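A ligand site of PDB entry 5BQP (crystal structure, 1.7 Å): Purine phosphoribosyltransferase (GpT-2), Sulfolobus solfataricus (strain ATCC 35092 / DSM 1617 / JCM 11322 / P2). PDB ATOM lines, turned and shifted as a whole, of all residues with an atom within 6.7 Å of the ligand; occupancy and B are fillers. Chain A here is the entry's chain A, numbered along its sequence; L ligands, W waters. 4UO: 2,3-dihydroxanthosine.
The side-chain carboxylate of Asp 94 is in hydrogen-bond range of an oxygen (O5') of the ligand, 2.5 Å away. O2 of the ligand sits close to OD2 of Asp 148, 2.6 Å away. The backbone NH (N) of Ile 143 is in hydrogen-bond range of an oxygen (O6) of the ligand (2.8 Å). The backbone carbonyl oxygen (O) of Ile 143 is in hydrogen-bond range of a nitrogen (N1) of the ligand, at 2.7 Å. NZ of Lys 125 sits at hydrogen-bond distance from O6 of the ligand, 2.7 Å away.
The indole nitrogen of Trp 147 sits at hydrogen-bond distance from the side-chain carboxylate of Asp 94 (3.0 Å). OD1 of Asp 148 sits at hydrogen-bond distance from N of Phe 145, 2.9 Å away. The side-chain carboxylate of Asp 97 is in salt-bridge range of the side-chain amino group of Lys 125 (2.7 Å). O of Ala 96 is in hydrogen-bond range of N of Lys 125, at 3.0 Å. The side-chain carboxylate (OD1) of Asp 93 lies within hydrogen-bond range of the backbone NH (N) of Gly 40, at 3.5 Å.
A nitrogen (N7) of the ligand sits close to the side-chain carboxylate (OD2) of Asp 97 (2.9 Å). N1 of the ligand lies close to NE1 of Trp 142 (3.5 Å). Residues that only touch the ligand: Val 95, Asp 93, Phe 145 and Phe 63. Ten residues have an atom within 4 Å of the ligand: Phe 63, Asp 93, Asp 94, Val 95, Asp 97, Lys 125, Trp 142, Ile 143, Phe 145 and Asp 148.
Water W1 lies within hydrogen-bond range of the side-chain carboxylate (OD1) of Asp 93 (2.6 Å), an oxygen (O5') of the ligand (2.8 Å) and the backbone NH (N) of Gly 39 (3.0 Å). Water W4 lies within hydrogen-bond range of OD2 of Asp 93 (2.7 Å), O5' of the ligand (3.0 Å) and O of Val 95 (3.1 Å). Water W3 bridges the side-chain carboxylate (OD2) of Asp 94 (2.6 Å) and the side-chain carboxylate (OD2) of Asp 148 (2.8 Å).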
ATOM      1  N   VAL A  36      15.545  -6.481  28.960  1.00  0.00           N
ATOM      2  CA  VAL A  36      15.259  -7.249  27.758  1.00  0.00           C
ATOM      3  C   VAL A  36      14.002  -8.066  27.966  1.00  0.00           C
ATOM      4  O   VAL A  36      13.998  -8.936  28.834  1.00  0.00           O
ATOM      5  CB  VAL A  36      16.436  -8.193  27.435  1.00  0.00           C
ATOM      6  CG1 VAL A  36      16.082  -9.053  26.195  1.00  0.00           C
ATOM      7  CG2 VAL A  36      17.696  -7.374  27.211  1.00  0.00           C
ATOM      8  N   LEU A  37      12.915  -7.772  27.239  1.00  0.00           N
ATOM      9  CA  LEU A  37      11.656  -8.523  27.419  1.00  0.00           C
ATOM     10  C   LEU A  37      11.738  -9.870  26.721  1.00  0.00           C
ATOM     11  O   LEU A  37      12.247  -9.910  25.601  1.00  0.00           O
ATOM     12  CB  LEU A  37      10.461  -7.739  26.856  1.00  0.00           C
ATOM     13  CG  LEU A  37      10.250  -6.327  27.417  1.00  0.00           C
ATOM     14  CD1 LEU A  37       9.100  -5.661  26.693  1.00  0.00           C
ATOM     15  CD2 LEU A  37       9.858  -6.457  28.895  1.00  0.00           C
ATOM     16  N   THR A  38      11.267 -10.964  27.355  1.00  0.00           N
ATOM     17  CA  THR A  38      10.650 -10.916  28.690  1.00  0.00           C
ATOM     18  C   THR A  38      11.527 -11.599  29.743  1.00  0.00           C
ATOM     19  O   THR A  38      11.198 -11.597  30.925  1.00  0.00           O
ATOM     20  CB  THR A  38       9.249 -11.621  28.708  1.00  0.00           C
ATOM     21  OG1 THR A  38       9.427 -12.980  28.291  1.00  0.00           O
ATOM     22  CG2 THR A  38       8.247 -10.892  27.744  1.00  0.00           C
ATOM     23  N   GLY A  39      12.632 -12.210  29.322  1.00  0.00           N
ATOM     24  CA  GLY A  39      13.503 -12.928  30.258  1.00  0.00           C
ATOM     25  C   GLY A  39      14.202 -11.987  31.251  1.00  0.00           C
ATOM     26  O   GLY A  39      14.520 -12.382  32.374  1.00  0.00           O
ATOM     27  N   GLY A  40      14.405 -10.729  30.854  1.00  0.00           N
ATOM     28  CA  GLY A  40      15.123  -9.776  31.697  1.00  0.00           C
ATOM     29  C   GLY A  40      14.213  -9.062  32.694  1.00  0.00           C
ATOM     30  O   GLY A  40      14.711  -8.289  33.540  1.00  0.00           O
ATOM     31  N   LYS A  62      12.909 -10.759  20.357  1.00  0.00           N
ATOM     32  CA  LYS A  62      12.705 -12.199  20.360  1.00  0.00           C
ATOM     33  C   LYS A  62      13.720 -12.873  19.451  1.00  0.00           C
ATOM     34  O   LYS A  62      14.005 -12.369  18.365  1.00  0.00           O
ATOM     35  CB  LYS A  62      11.288 -12.553  19.916  1.00  0.00           C
ATOM     36  CG  LYS A  62      10.237 -12.371  20.999  1.00  0.00           C
ATOM     37  CD  LYS A  62      10.164 -13.602  21.889  1.00  0.00           C
ATOM     38  CE  LYS A  62       8.840 -13.671  22.643  1.00  0.00           C
ATOM     39  NZ  LYS A  62       8.814 -12.889  23.908  1.00  0.00           N
ATOM     40  N   PHE A  63      14.256 -13.990  19.912  1.00  0.00           N
ATOM     41  CA  PHE A  63      15.241 -14.735  19.139  1.00  0.00           C
ATOM     42  C   PHE A  63      14.760 -16.175  18.944  1.00  0.00           C
ATOM     43  O   PHE A  63      14.860 -16.970  19.879  1.00  0.00           O
ATOM     44  CB  PHE A  63      16.593 -14.707  19.854  1.00  0.00           C
ATOM     45  CG  PHE A  63      17.721 -15.325  19.075  1.00  0.00           C
ATOM     46  CD1 PHE A  63      17.585 -15.630  17.733  1.00  0.00           C
ATOM     47  CD2 PHE A  63      18.929 -15.609  19.689  1.00  0.00           C
ATOM     48  CE1 PHE A  63      18.627 -16.205  17.026  1.00  0.00           C
ATOM     49  CE2 PHE A  63      19.978 -16.172  18.986  1.00  0.00           C
ATOM     50  CZ  PHE A  63      19.825 -16.479  17.658  1.00  0.00           C
ATOM     51  N   ASP A  93      19.435  -8.871  31.160  1.00  0.00           N
ATOM     52  CA  ASP A  93      18.750 -10.064  30.656  1.00  0.00           C
ATOM     53  C   ASP A  93      18.968 -11.217  31.619  1.00  0.00           C
ATOM     54  O   ASP A  93      19.785 -11.130  32.552  1.00  0.00           O
ATOM     55  CB  ASP A  93      19.291 -10.410  29.254  1.00  0.00           C
ATOM     56  CG  ASP A  93      18.255 -11.149  28.373  1.00  0.00           C
ATOM     57  OD1 ASP A  93      17.129 -11.458  28.836  1.00  0.00           O
ATOM     58  OD2 ASP A  93      18.596 -11.461  27.186  1.00  0.00           O
ATOM     59  N   ASP A  94      18.286 -12.340  31.396  1.00  0.00           N
ATOM     60  CA  ASP A  94      18.473 -13.469  32.298  1.00  0.00           C
ATOM     61  C   ASP A  94      19.657 -14.351  31.887  1.00  0.00           C
ATOM     62  O   ASP A  94      20.380 -14.801  32.751  1.00  0.00           O
ATOM     63  CB  ASP A  94      17.203 -14.313  32.485  1.00  0.00           C
ATOM     64  CG  ASP A  94      16.527 -14.746  31.192  1.00  0.00           C
ATOM     65  OD1 ASP A  94      16.996 -14.502  30.054  1.00  0.00           O
ATOM     66  OD2 ASP A  94      15.429 -15.345  31.357  1.00  0.00           O
ATOM     67  N   VAL A  95      19.841 -14.615  30.591  1.00  0.00           N
ATOM     68  CA  VAL A  95      20.958 -15.492  30.193  1.00  0.00           C
ATOM     69  C   VAL A  95      21.584 -14.940  28.912  1.00  0.00           C
ATOM     70  O   VAL A  95      20.866 -14.454  28.033  1.00  0.00           O
ATOM     71  CB  VAL A  95      20.479 -16.973  30.008  1.00  0.00           C
ATOM     72  CG1 VAL A  95      19.333 -17.043  28.981  1.00  0.00           C
ATOM     73  CG2 VAL A  95      21.662 -17.899  29.570  1.00  0.00           C
ATOM     74  N   ALA A  96      22.905 -14.980  28.831  1.00  0.00           N
ATOM     75  CA  ALA A  96      23.577 -14.768  27.539  1.00  0.00           C
ATOM     76  C   ALA A  96      24.050 -16.137  27.031  1.00  0.00           C
ATOM     77  O   ALA A  96      24.947 -16.746  27.629  1.00  0.00           O
ATOM     78  CB  ALA A  96      24.741 -13.794  27.678  1.00  0.00           C
ATOM     79  N   ASP A  97      23.436 -16.620  25.938  1.00  0.00           N
ATOM     80  CA  ASP A  97      23.756 -17.924  25.391  1.00  0.00           C
ATOM     81  C   ASP A  97      24.580 -17.737  24.128  1.00  0.00           C
ATOM     82  O   ASP A  97      25.802 -17.855  24.162  1.00  0.00           O
ATOM     83  CB  ASP A  97      22.501 -18.717  25.093  1.00  0.00           C
ATOM     84  CG  ASP A  97      22.798 -20.185  24.753  1.00  0.00           C
ATOM     85  OD1 ASP A  97      23.561 -20.416  23.809  1.00  0.00           O
ATOM     86  OD2 ASP A  97      22.297 -21.108  25.418  1.00  0.00           O
ATOM     87  N   THR A  98      23.914 -17.396  23.024  1.00  0.00           N
ATOM     88  CA  THR A  98      24.677 -17.108  21.795  1.00  0.00           C
ATOM     89  C   THR A  98      25.301 -15.732  21.919  1.00  0.00           C
ATOM     90  O   THR A  98      26.305 -15.436  21.268  1.00  0.00           O
ATOM     91  CB  THR A  98      23.825 -17.122  20.518  1.00  0.00           C
ATOM     92  OG1 THR A  98      22.846 -16.069  20.548  1.00  0.00           O
ATOM     93  CG2 THR A  98      23.137 -18.458  20.330  1.00  0.00           C
ATOM     94  N   THR A 101      21.374 -11.675  21.407  1.00  0.00           N
ATOM     95  CA  THR A 101      20.404 -10.734  21.998  1.00  0.00           C
ATOM     96  C   THR A 101      21.105  -9.520  22.588  1.00  0.00           C
ATOM     97  O   THR A 101      20.733  -8.380  22.277  1.00  0.00           O
ATOM     98  CB  THR A 101      19.542 -11.422  23.060  1.00  0.00           C
ATOM     99  OG1 THR A 101      18.767 -12.430  22.434  1.00  0.00           O
ATOM    100  CG2 THR A 101      18.570 -10.388  23.718  1.00  0.00           C
ATOM    101  N   LYS A 125      26.792 -18.438  29.213  1.00  0.00           N
ATOM    102  CA  LYS A 125      27.328 -19.678  28.619  1.00  0.00           C
ATOM    103  C   LYS A 125      28.751 -19.411  28.125  1.00  0.00           C
ATOM    104  O   LYS A 125      29.024 -18.342  27.616  1.00  0.00           O
ATOM    105  CB  LYS A 125      26.437 -20.162  27.460  1.00  0.00           C
ATOM    106  CG  LYS A 125      24.975 -20.356  27.848  1.00  0.00           C
ATOM    107  CD  LYS A 125      24.751 -21.496  28.874  1.00  0.00           C
ATOM    108  CE  LYS A 125      23.239 -21.603  29.187  1.00  0.00           C
ATOM    109  NZ  LYS A 125      22.451 -22.055  27.989  1.00  0.00           N
ATOM    110  N   LYS A 141      25.152 -25.786  31.258  1.00  0.00           N
ATOM    111  CA  LYS A 141      23.863 -26.487  31.172  1.00  0.00           C
ATOM    112  C   LYS A 141      22.745 -25.577  30.657  1.00  0.00           C
ATOM    113  O   LYS A 141      22.849 -24.382  30.762  1.00  0.00           O
ATOM    114  CB  LYS A 141      23.461 -27.028  32.546  1.00  0.00           C
ATOM    115  CG  LYS A 141      24.533 -27.909  33.221  1.00  0.00           C
ATOM    116  CD  LYS A 141      23.908 -28.891  34.198  1.00  0.00           C
ATOM    117  CE  LYS A 141      24.982 -29.816  34.791  1.00  0.00           C
ATOM    118  NZ  LYS A 141      25.340 -29.392  36.172  1.00  0.00           N
ATOM    119  N   TRP A 142      21.664 -26.162  30.137  1.00  0.00           N
ATOM    120  CA  TRP A 142      20.471 -25.347  29.840  1.00  0.00           C
ATOM    121  C   TRP A 142      19.830 -24.906  31.166  1.00  0.00           C
ATOM    122  O   TRP A 142      19.551 -25.720  32.030  1.00  0.00           O
ATOM    123  CB  TRP A 142      19.453 -26.115  29.004  1.00  0.00           C
ATOM    124  CG  TRP A 142      18.304 -25.245  28.433  1.00  0.00           C
ATOM    125  CD1 TRP A 142      17.019 -25.117  28.906  1.00  0.00           C
ATOM    126  CD2 TRP A 142      18.397 -24.393  27.289  1.00  0.00           C
ATOM    127  NE1 TRP A 142      16.306 -24.236  28.114  1.00  0.00           N
ATOM    128  CE2 TRP A 142      17.134 -23.778  27.116  1.00  0.00           C
ATOM    129  CE3 TRP A 142      19.425 -24.085  26.381  1.00  0.00           C
ATOM    130  CZ2 TRP A 142      16.875 -22.881  26.071  1.00  0.00           C
ATOM    131  CZ3 TRP A 142      19.169 -23.189  25.360  1.00  0.00           C
ATOM    132  CH2 TRP A 142      17.900 -22.597  25.211  1.00  0.00           C
ATOM    133  N   ILE A 143      19.571 -23.615  31.301  1.00  0.00           N
ATOM    134  CA  ILE A 143      19.010 -23.116  32.534  1.00  0.00           C
ATOM    135  C   ILE A 143      17.494 -23.100  32.477  1.00  0.00           C
ATOM    136  O   ILE A 143      16.906 -22.647  31.489  1.00  0.00           O
ATOM    137  CB  ILE A 143      19.529 -21.694  32.834  1.00  0.00           C
ATOM    138  CG1 ILE A 143      21.050 -21.732  32.894  1.00  0.00           C
ATOM    139  CG2 ILE A 143      18.978 -21.161  34.155  1.00  0.00           C
ATOM    140  CD1 ILE A 143      21.616 -20.438  32.496  1.00  0.00           C
ATOM    141  N   ILE A 144      16.834 -23.629  33.504  1.00  0.00           N
ATOM    142  CA  ILE A 144      15.381 -23.491  33.611  1.00  0.00           C
ATOM    143  C   ILE A 144      15.115 -22.388  34.653  1.00  0.00           C
ATOM    144  O   ILE A 144      15.337 -22.597  35.816  1.00  0.00           O
ATOM    145  CB  ILE A 144      14.681 -24.798  34.029  1.00  0.00           C
ATOM    146  CG1 ILE A 144      15.094 -25.900  33.051  1.00  0.00           C
ATOM    147  CG2 ILE A 144      13.145 -24.650  33.990  1.00  0.00           C
ATOM    148  CD1 ILE A 144      14.319 -27.216  33.308  1.00  0.00           C
ATOM    149  N   PHE A 145      14.677 -21.207  34.201  1.00  0.00           N
ATOM    150  CA  PHE A 145      14.357 -20.151  35.157  1.00  0.00           C
ATOM    151  C   PHE A 145      13.016 -20.324  35.783  1.00  0.00           C
ATOM    152  O   PHE A 145      12.110 -20.910  35.200  1.00  0.00           O
ATOM    153  CB  PHE A 145      14.412 -18.785  34.454  1.00  0.00           C
ATOM    154  CG  PHE A 145      15.813 -18.391  33.996  1.00  0.00           C
ATOM    155  CD1 PHE A 145      16.733 -17.859  34.882  1.00  0.00           C
ATOM    156  CD2 PHE A 145      16.184 -18.568  32.670  1.00  0.00           C
ATOM    157  CE1 PHE A 145      18.021 -17.482  34.441  1.00  0.00           C
ATOM    158  CE2 PHE A 145      17.449 -18.195  32.235  1.00  0.00           C
ATOM    159  CZ  PHE A 145      18.372 -17.679  33.137  1.00  0.00           C
ATOM    160  N   TRP A 147      10.767 -18.307  35.930  1.00  0.00           N
ATOM    161  CA  TRP A 147       9.788 -17.556  35.137  1.00  0.00           C
ATOM    162  C   TRP A 147       9.643 -18.077  33.716  1.00  0.00           C
ATOM    163  O   TRP A 147       8.881 -17.537  32.924  1.00  0.00           O
ATOM    164  CB  TRP A 147      10.167 -16.048  35.080  1.00  0.00           C
ATOM    165  CG  TRP A 147      11.591 -15.783  34.742  1.00  0.00           C
ATOM    166  CD1 TRP A 147      12.182 -15.750  33.486  1.00  0.00           C
ATOM    167  CD2 TRP A 147      12.655 -15.591  35.684  1.00  0.00           C
ATOM    168  NE1 TRP A 147      13.522 -15.466  33.617  1.00  0.00           N
ATOM    169  CE2 TRP A 147      13.835 -15.350  34.946  1.00  0.00           C
ATOM    170  CE3 TRP A 147      12.709 -15.515  37.075  1.00  0.00           C
ATOM    171  CZ2 TRP A 147      15.074 -15.112  35.565  1.00  0.00           C
ATOM    172  CZ3 TRP A 147      13.923 -15.256  37.682  1.00  0.00           C
ATOM    173  CH2 TRP A 147      15.081 -15.074  36.951  1.00  0.00           C
ATOM    174  N   ASP A 148      10.433 -19.100  33.331  1.00  0.00           N
ATOM    175  CA  ASP A 148      10.162 -19.712  32.011  1.00  0.00           C
ATOM    176  C   ASP A 148      10.120 -21.227  32.113  1.00  0.00           C
ATOM    177  O   ASP A 148      10.170 -21.898  31.075  1.00  0.00           O
ATOM    178  CB  ASP A 148      11.152 -19.248  30.906  1.00  0.00           C
ATOM    179  CG  ASP A 148      12.577 -19.789  31.061  1.00  0.00           C
ATOM    180  OD1 ASP A 148      12.944 -20.494  32.006  1.00  0.00           O
ATOM    181  OD2 ASP A 148      13.383 -19.449  30.165  1.00  0.00           O
ATOM    182  N   ASP A 151       7.427 -22.666  29.867  1.00  0.00           N
ATOM    183  CA  ASP A 151       7.895 -22.630  28.486  1.00  0.00           C
ATOM    184  C   ASP A 151       8.858 -23.797  28.224  1.00  0.00           C
ATOM    185  O   ASP A 151       8.781 -24.451  27.178  1.00  0.00           O
ATOM    186  CB  ASP A 151       8.564 -21.306  28.180  1.00  0.00           C
ATOM    187  CG  ASP A 151       8.228 -20.842  26.817  1.00  0.00           C
ATOM    188  OD1 ASP A 151       7.050 -20.448  26.647  1.00  0.00           O
ATOM    189  OD2 ASP A 151       9.101 -20.906  25.923  1.00  0.00           O
ATOM    190  N   VAL A 152       9.773 -24.049  29.143  1.00  0.00           N
ATOM    191  CA  VAL A 152      10.690 -25.166  28.931  1.00  0.00           C
ATOM    192  C   VAL A 152       9.924 -26.498  28.911  1.00  0.00           C
ATOM    193  O   VAL A 152      10.184 -27.350  28.054  1.00  0.00           O
ATOM    194  CB  VAL A 152      11.790 -25.193  29.995  1.00  0.00           C
ATOM    195  CG1 VAL A 152      12.727 -26.423  29.811  1.00  0.00           C
ATOM    196  CG2 VAL A 152      12.620 -23.914  29.861  1.00  0.00           C
HETATM  197  O6  4UO L   1      19.999 -21.885  29.126  1.00  0.00           O
HETATM  198  C6  4UO L   1      18.881 -21.172  28.665  1.00  0.00           C
HETATM  199  N1  4UO L   1      17.749 -21.307  29.309  1.00  0.00           N
HETATM  200  C2  4UO L   1      16.629 -20.706  28.919  1.00  0.00           C
HETATM  201  O2  4UO L   1      15.517 -20.935  29.691  1.00  0.00           O
HETATM  202  N3  4UO L   1      16.572 -19.929  27.851  1.00  0.00           N
HETATM  203  C4  4UO L   1      17.707 -19.721  27.145  1.00  0.00           C
HETATM  204  C5  4UO L   1      18.908 -20.349  27.502  1.00  0.00           C
HETATM  205  N7  4UO L   1      19.862 -19.983  26.598  1.00  0.00           N
HETATM  206  C8  4UO L   1      19.259 -19.156  25.719  1.00  0.00           C
HETATM  207  N9  4UO L   1      17.981 -18.986  26.005  1.00  0.00           N
HETATM  208  C1' 4UO L   1      17.057 -18.089  25.272  1.00  0.00           C
HETATM  209  O4' 4UO L   1      16.840 -16.941  26.093  1.00  0.00           O
HETATM  210  C4' 4UO L   1      15.414 -16.668  26.168  1.00  0.00           C
HETATM  211  C5' 4UO L   1      15.067 -15.986  27.482  1.00  0.00           C
HETATM  212  O5' 4UO L   1      15.976 -14.938  27.806  1.00  0.00           O
HETATM  213  C3' 4UO L   1      14.777 -18.032  25.961  1.00  0.00           C
HETATM  214  O3' 4UO L   1      13.414 -17.930  25.560  1.00  0.00           O
HETATM  215  C2' 4UO L   1      15.698 -18.697  24.929  1.00  0.00           C
HETATM  216  O2' 4UO L   1      15.363 -18.287  23.619  1.00  0.00           O
HETATM  217  O   HOH W   1      15.045 -12.312  27.477  1.00  0.00           O
HETATM  218  O   HOH W   2      16.957 -15.922  23.115  1.00  0.00           O
HETATM  219  O   HOH W   3      13.544 -16.635  30.218  1.00  0.00           O
HETATM  220  O   HOH W   4      18.344 -14.000  26.214  1.00  0.00           O
